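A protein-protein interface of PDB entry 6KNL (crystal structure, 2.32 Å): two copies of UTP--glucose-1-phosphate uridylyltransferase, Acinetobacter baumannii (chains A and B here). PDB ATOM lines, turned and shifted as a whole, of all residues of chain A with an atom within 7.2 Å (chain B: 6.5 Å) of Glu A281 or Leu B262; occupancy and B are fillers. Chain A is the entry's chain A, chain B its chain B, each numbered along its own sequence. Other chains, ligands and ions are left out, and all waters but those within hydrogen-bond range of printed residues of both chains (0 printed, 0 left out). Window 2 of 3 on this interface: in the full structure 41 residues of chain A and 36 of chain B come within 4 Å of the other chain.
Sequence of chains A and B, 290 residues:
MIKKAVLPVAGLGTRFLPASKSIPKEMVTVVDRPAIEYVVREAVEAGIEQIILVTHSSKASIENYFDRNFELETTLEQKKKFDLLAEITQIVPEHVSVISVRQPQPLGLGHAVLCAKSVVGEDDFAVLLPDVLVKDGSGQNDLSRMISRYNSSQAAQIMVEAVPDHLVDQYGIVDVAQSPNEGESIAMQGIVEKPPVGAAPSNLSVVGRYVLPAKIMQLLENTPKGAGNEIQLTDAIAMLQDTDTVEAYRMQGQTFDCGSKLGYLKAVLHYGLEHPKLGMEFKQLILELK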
ATOM      1  N   LYS A 277      17.554 -16.351 -18.958  1.00  0.00           N
ATOM      2  CA  LYS A 277      18.470 -17.291 -19.671  1.00  0.00           C
ATOM      3  C   LYS A 277      18.219 -18.757 -19.280  1.00  0.00           C
ATOM      4  O   LYS A 277      18.357 -19.632 -20.169  1.00  0.00           O
ATOM      5  CB  LYS A 277      19.930 -16.946 -19.370  1.00  0.00           C
ATOM      6  CG  LYS A 277      20.506 -15.787 -20.170  1.00  0.00           C
ATOM      7  CD  LYS A 277      21.358 -16.224 -21.348  1.00  0.00           C
ATOM      8  CE  LYS A 277      21.733 -15.088 -22.278  1.00  0.00           C
ATOM      9  NZ  LYS A 277      22.076 -13.853 -21.535  1.00  0.00           N
ATOM     10  N   LEU A 278      17.896 -19.030 -18.014  1.00  0.00           N
ATOM     11  CA  LEU A 278      17.823 -20.413 -17.467  1.00  0.00           C
ATOM     12  C   LEU A 278      16.377 -20.885 -17.374  1.00  0.00           C
ATOM     13  O   LEU A 278      16.195 -22.095 -17.213  1.00  0.00           O
ATOM     14  CB  LEU A 278      18.449 -20.453 -16.071  1.00  0.00           C
ATOM     15  CG  LEU A 278      19.856 -19.879 -15.957  1.00  0.00           C
ATOM     16  CD1 LEU A 278      20.161 -19.543 -14.510  1.00  0.00           C
ATOM     17  CD2 LEU A 278      20.888 -20.838 -16.527  1.00  0.00           C
ATOM     18  N   GLY A 279      15.405 -19.967 -17.411  1.00  0.00           N
ATOM     19  CA  GLY A 279      14.005 -20.250 -17.037  1.00  0.00           C
ATOM     20  C   GLY A 279      13.491 -21.527 -17.683  1.00  0.00           C
ATOM     21  O   GLY A 279      13.044 -22.437 -16.947  1.00  0.00           O
ATOM     22  N   MET A 280      13.579 -21.600 -19.013  1.00  0.00           N
ATOM     23  CA  MET A 280      13.049 -22.727 -19.825  1.00  0.00           C
ATOM     24  C   MET A 280      13.677 -24.033 -19.337  1.00  0.00           C
ATOM     25  O   MET A 280      12.917 -24.941 -18.952  1.00  0.00           O
ATOM     26  CB  MET A 280      13.356 -22.538 -21.315  1.00  0.00           C
ATOM     27  CG  MET A 280      12.580 -21.401 -21.968  1.00  0.00           C
ATOM     28  SD  MET A 280      10.959 -21.910 -22.595  1.00  0.00           S
ATOM     29  CE  MET A 280       9.906 -21.499 -21.201  1.00  0.00           C
ATOM     30  N   GLU A 281      15.009 -24.113 -19.336  1.00  0.00           N
ATOM     31  CA  GLU A 281      15.749 -25.353 -18.976  1.00  0.00           C
ATOM     32  C   GLU A 281      15.491 -25.698 -17.507  1.00  0.00           C
ATOM     33  O   GLU A 281      15.574 -26.888 -17.168  1.00  0.00           O
ATOM     34  CB  GLU A 281      17.250 -25.211 -19.203  1.00  0.00           C
ATOM     35  CG  GLU A 281      17.655 -25.131 -20.662  1.00  0.00           C
ATOM     36  CD  GLU A 281      18.980 -24.401 -20.859  1.00  0.00           C
ATOM     37  OE1 GLU A 281      18.991 -23.143 -20.739  1.00  0.00           O
ATOM     38  OE2 GLU A 281      20.007 -25.089 -21.077  1.00  0.00           O
ATOM     39  N   PHE A 282      15.191 -24.706 -16.665  1.00  0.00           N
ATOM     40  CA  PHE A 282      14.855 -24.934 -15.236  1.00  0.00           C
ATOM     41  C   PHE A 282      13.478 -25.603 -15.151  1.00  0.00           C
ATOM     42  O   PHE A 282      13.383 -26.661 -14.552  1.00  0.00           O
ATOM     43  CB  PHE A 282      14.945 -23.632 -14.445  1.00  0.00           C
ATOM     44  CG  PHE A 282      14.690 -23.808 -12.976  1.00  0.00           C
ATOM     45  CD1 PHE A 282      15.443 -24.702 -12.234  1.00  0.00           C
ATOM     46  CD2 PHE A 282      13.706 -23.077 -12.338  1.00  0.00           C
ATOM     47  CE1 PHE A 282      15.212 -24.858 -10.878  1.00  0.00           C
ATOM     48  CE2 PHE A 282      13.468 -23.242 -10.983  1.00  0.00           C
ATOM     49  CZ  PHE A 282      14.227 -24.128 -10.256  1.00  0.00           C
ATOM     50  N   LYS A 283      12.457 -25.029 -15.787  1.00  0.00           N
ATOM     51  CA  LYS A 283      11.108 -25.650 -15.935  1.00  0.00           C
ATOM     52  C   LYS A 283      11.260 -27.122 -16.349  1.00  0.00           C
ATOM     53  O   LYS A 283      10.527 -27.974 -15.798  1.00  0.00           O
ATOM     54  CB  LYS A 283      10.288 -24.863 -16.962  1.00  0.00           C
ATOM     55  CG  LYS A 283       9.034 -25.547 -17.506  1.00  0.00           C
ATOM     56  CD  LYS A 283       8.729 -25.189 -18.957  1.00  0.00           C
ATOM     57  CE  LYS A 283       7.294 -24.766 -19.188  1.00  0.00           C
ATOM     58  NZ  LYS A 283       7.120 -24.188 -20.541  1.00  0.00           N
ATOM     59  N   GLN A 284      12.179 -27.405 -17.278  1.00  0.00           N
ATOM     60  CA  GLN A 284      12.424 -28.763 -17.841  1.00  0.00           C
ATOM     61  C   GLN A 284      12.990 -29.670 -16.733  1.00  0.00           C
ATOM     62  O   GLN A 284      12.478 -30.796 -16.585  1.00  0.00           O
ATOM     63  CB  GLN A 284      13.334 -28.670 -19.072  1.00  0.00           C
ATOM     64  CG  GLN A 284      13.293 -29.898 -19.974  1.00  0.00           C
ATOM     65  CD  GLN A 284      11.978 -30.068 -20.701  1.00  0.00           C
ATOM     66  OE1 GLN A 284      11.488 -29.152 -21.358  1.00  0.00           O
ATOM     67  NE2 GLN A 284      11.400 -31.258 -20.599  1.00  0.00           N
ATOM     68  N   LEU A 285      13.977 -29.193 -15.962  1.00  0.00           N
ATOM     69  CA  LEU A 285      14.533 -29.929 -14.790  1.00  0.00           C
ATOM     70  C   LEU A 285      13.398 -30.280 -13.823  1.00  0.00           C
ATOM     71  O   LEU A 285      13.449 -31.382 -13.241  1.00  0.00           O
ATOM     72  CB  LEU A 285      15.600 -29.086 -14.082  1.00  0.00           C
ATOM     73  CG  LEU A 285      16.947 -28.957 -14.792  1.00  0.00           C
ATOM     74  CD1 LEU A 285      17.914 -28.134 -13.952  1.00  0.00           C
ATOM     75  CD2 LEU A 285      17.554 -30.317 -15.105  1.00  0.00           C
ATOM     76  N   ILE A 286      12.429 -29.371 -13.659  1.00  0.00           N
ATOM     77  CA  ILE A 286      11.221 -29.553 -12.800  1.00  0.00           C
ATOM     78  C   ILE A 286      10.400 -30.740 -13.326  1.00  0.00           C
ATOM     79  O   ILE A 286      10.236 -31.710 -12.561  1.00  0.00           O
ATOM     80  CB  ILE A 286      10.376 -28.266 -12.748  1.00  0.00           C
ATOM     81  CG1 ILE A 286      10.547 -27.525 -11.421  1.00  0.00           C
ATOM     82  CD1 ILE A 286      11.716 -26.576 -11.416  1.00  0.00           C
ATOM     83  N   GLU A 288      10.942 -33.272 -15.291  1.00  0.00           N
ATOM     84  CA  GLU A 288      11.683 -34.562 -15.261  1.00  0.00           C
ATOM     85  C   GLU A 288      11.673 -35.185 -13.856  1.00  0.00           C
ATOM     86  O   GLU A 288      12.037 -36.371 -13.760  1.00  0.00           O
ATOM     87  CB  GLU A 288      13.118 -34.338 -15.747  1.00  0.00           C
ATOM     88  CG  GLU A 288      13.214 -33.944 -17.215  1.00  0.00           C
ATOM     89  CD  GLU A 288      14.505 -33.249 -17.617  1.00  0.00           C
ATOM     90  OE1 GLU A 288      15.516 -33.409 -16.892  1.00  0.00           O
ATOM     91  OE2 GLU A 288      14.499 -32.546 -18.651  1.00  0.00           O
ATOM     92  N   PHE B  16      30.471 -20.228 -11.925  1.00  0.00           N
ATOM     93  CA  PHE B  16      29.251 -19.940 -11.123  1.00  0.00           C
ATOM     94  C   PHE B  16      29.288 -18.488 -10.632  1.00  0.00           C
ATOM     95  O   PHE B  16      28.913 -18.190  -9.489  1.00  0.00           O
ATOM     96  CB  PHE B  16      28.997 -20.991 -10.032  1.00  0.00           C
ATOM     97  CG  PHE B  16      27.539 -21.023  -9.639  1.00  0.00           C
ATOM     98  CD1 PHE B  16      26.552 -21.221 -10.595  1.00  0.00           C
ATOM     99  CD2 PHE B  16      27.145 -20.749  -8.340  1.00  0.00           C
ATOM    100  CE1 PHE B  16      25.209 -21.187 -10.251  1.00  0.00           C
ATOM    101  CE2 PHE B  16      25.800 -20.713  -8.000  1.00  0.00           C
ATOM    102  CZ  PHE B  16      24.835 -20.935  -8.956  1.00  0.00           C
ATOM    103  N   ASP B 257      27.254 -31.083 -11.070  1.00  0.00           N
ATOM    104  CA  ASP B 257      28.308 -30.041 -11.180  1.00  0.00           C
ATOM    105  C   ASP B 257      27.709 -28.758 -10.602  1.00  0.00           C
ATOM    106  O   ASP B 257      26.874 -28.164 -11.296  1.00  0.00           O
ATOM    107  CB  ASP B 257      28.791 -29.877 -12.628  1.00  0.00           C
ATOM    108  CG  ASP B 257      30.026 -29.001 -12.803  1.00  0.00           C
ATOM    109  OD1 ASP B 257      30.521 -28.451 -11.802  1.00  0.00           O
ATOM    110  OD2 ASP B 257      30.495 -28.879 -13.955  1.00  0.00           O
ATOM    111  N   GLY B 259      29.193 -26.069 -10.219  1.00  0.00           N
ATOM    112  CA  GLY B 259      29.889 -24.979 -10.926  1.00  0.00           C
ATOM    113  C   GLY B 259      29.128 -24.564 -12.173  1.00  0.00           C
ATOM    114  O   GLY B 259      29.230 -23.383 -12.551  1.00  0.00           O
ATOM    115  N   SER B 260      28.401 -25.497 -12.799  1.00  0.00           N
ATOM    116  CA  SER B 260      27.490 -25.229 -13.941  1.00  0.00           C
ATOM    117  C   SER B 260      26.120 -24.816 -13.380  1.00  0.00           C
ATOM    118  O   SER B 260      25.639 -25.477 -12.432  1.00  0.00           O
ATOM    119  CB  SER B 260      27.415 -26.408 -14.884  1.00  0.00           C
ATOM    120  OG  SER B 260      26.221 -27.159 -14.718  1.00  0.00           O
ATOM    121  N   LYS B 261      25.535 -23.740 -13.918  1.00  0.00           N
ATOM    122  CA  LYS B 261      24.333 -23.072 -13.344  1.00  0.00           C
ATOM    123  C   LYS B 261      23.172 -24.072 -13.295  1.00  0.00           C
ATOM    124  O   LYS B 261      22.464 -24.073 -12.269  1.00  0.00           O
ATOM    125  CB  LYS B 261      24.009 -21.781 -14.103  1.00  0.00           C
ATOM    126  CG  LYS B 261      24.873 -20.595 -13.695  1.00  0.00           C
ATOM    127  CD  LYS B 261      24.634 -19.363 -14.522  1.00  0.00           C
ATOM    128  CE  LYS B 261      25.296 -18.124 -13.948  1.00  0.00           C
ATOM    129  NZ  LYS B 261      24.668 -16.878 -14.459  1.00  0.00           N
ATOM    130  N   LEU B 262      23.046 -24.924 -14.322  1.00  0.00           N
ATOM    131  CA  LEU B 262      22.002 -25.986 -14.438  1.00  0.00           C
ATOM    132  C   LEU B 262      22.314 -27.185 -13.530  1.00  0.00           C
ATOM    133  O   LEU B 262      21.365 -27.765 -12.994  1.00  0.00           O
ATOM    134  CB  LEU B 262      21.891 -26.433 -15.900  1.00  0.00           C
ATOM    135  CG  LEU B 262      20.638 -25.998 -16.659  1.00  0.00           C
ATOM    136  CD1 LEU B 262      20.056 -24.691 -16.133  1.00  0.00           C
ATOM    137  CD2 LEU B 262      20.951 -25.861 -18.134  1.00  0.00           C
ATOM    138  N   GLY B 263      23.583 -27.567 -13.392  1.00  0.00           N
ATOM    139  CA  GLY B 263      24.014 -28.601 -12.430  1.00  0.00           C
ATOM    140  C   GLY B 263      23.685 -28.214 -10.995  1.00  0.00           C
ATOM    141  O   GLY B 263      23.242 -29.088 -10.243  1.00  0.00           O
ATOM    142  N   TYR B 264      23.904 -26.954 -10.617  1.00  0.00           N
ATOM    143  CA  TYR B 264      23.552 -26.409  -9.280  1.00  0.00           C
ATOM    144  C   TYR B 264      22.024 -26.398  -9.118  1.00  0.00           C
ATOM    145  O   TYR B 264      21.531 -26.945  -8.118  1.00  0.00           O
ATOM    146  CB  TYR B 264      24.173 -25.028  -9.065  1.00  0.00           C
ATOM    147  CG  TYR B 264      23.555 -24.214  -7.956  1.00  0.00           C
ATOM    148  CD1 TYR B 264      22.482 -23.388  -8.197  1.00  0.00           C
ATOM    149  CD2 TYR B 264      24.068 -24.254  -6.674  1.00  0.00           C
ATOM    150  CE1 TYR B 264      21.923 -22.619  -7.192  1.00  0.00           C
ATOM    151  CE2 TYR B 264      23.507 -23.516  -5.644  1.00  0.00           C
ATOM    152  CZ  TYR B 264      22.429 -22.690  -5.905  1.00  0.00           C
ATOM    153  OH  TYR B 264      21.879 -21.951  -4.900  1.00  0.00           O
ATOM    154  N   LEU B 265      21.284 -25.846 -10.081  1.00  0.00           N
ATOM    155  CA  LEU B 265      19.792 -25.828 -10.029  1.00  0.00           C
ATOM    156  C   LEU B 265      19.251 -27.262  -9.875  1.00  0.00           C
ATOM    157  O   LEU B 265      18.170 -27.423  -9.265  1.00  0.00           O
ATOM    158  CB  LEU B 265      19.212 -25.157 -11.284  1.00  0.00           C
ATOM    159  CG  LEU B 265      19.342 -23.634 -11.368  1.00  0.00           C
ATOM    160  CD1 LEU B 265      18.782 -22.972 -10.116  1.00  0.00           C
ATOM    161  N   LYS B 266      19.952 -28.269 -10.406  1.00  0.00           N
ATOM    162  CA  LYS B 266      19.485 -29.678 -10.376  1.00  0.00           C
ATOM    163  C   LYS B 266      19.741 -30.265  -8.992  1.00  0.00           C
ATOM    164  O   LYS B 266      18.904 -31.085  -8.541  1.00  0.00           O
ATOM    165  CB  LYS B 266      20.167 -30.544 -11.434  1.00  0.00           C
ATOM    166  CG  LYS B 266      19.525 -31.918 -11.613  1.00  0.00           C
ATOM    167  CD  LYS B 266      20.264 -32.857 -12.550  1.00  0.00           C
ATOM    168  CE  LYS B 266      19.420 -34.057 -12.927  1.00  0.00           C
ATOM    169  NZ  LYS B 266      20.255 -35.178 -13.412  1.00  0.00           N
ATOM    170  N   ALA B 267      20.845 -29.874  -8.353  1.00  0.00           N
ATOM    171  CA  ALA B 267      21.220 -30.333  -6.992  1.00  0.00           C
ATOM    172  C   ALA B 267      20.195 -29.810  -5.983  1.00  0.00           C
ATOM    173  O   ALA B 267      19.775 -30.584  -5.111  1.00  0.00           O
ATOM    174  CB  ALA B 267      22.610 -29.870  -6.632  1.00  0.00           C
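Among the printed residues, pairs that only touch across the chains: Leu A278 with Leu B262, Glu A281 with Leu B262, Phe A282 with Leu B265 and Leu A285 with Leu B262.
Of chain B, only Leu B262 comes within 4 Å of Glu A281.
Leu B262 touches just these residues of chain A: Leu A278, Glu A281 and Leu A285.
Printed residues of chain A within 4 Å of Leu B265: Phe A282.
Of the printed residues of chain B, Leu A285 touches Leu B262 (3.6 Å).
The nearest printed residue of chain B that does not touch Phe A282 is Leu B262 (4.9 Å).
Printed residues of chain A that touch a printed residue of chain B: Leu A278, Glu A281, Phe A282 and Leu A285.
Among the printed residues, 4 pairs touch across the chains.
Among the printed residues, no Asp or Glu carboxylate lies within 4 Å of a Lys or Arg side-chain nitrogen of the other chain.
No position is printed for both chains.
Of the 4 pairs that touch across the chains among the printed residues, none has its exchanged pair printed and touching as well.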
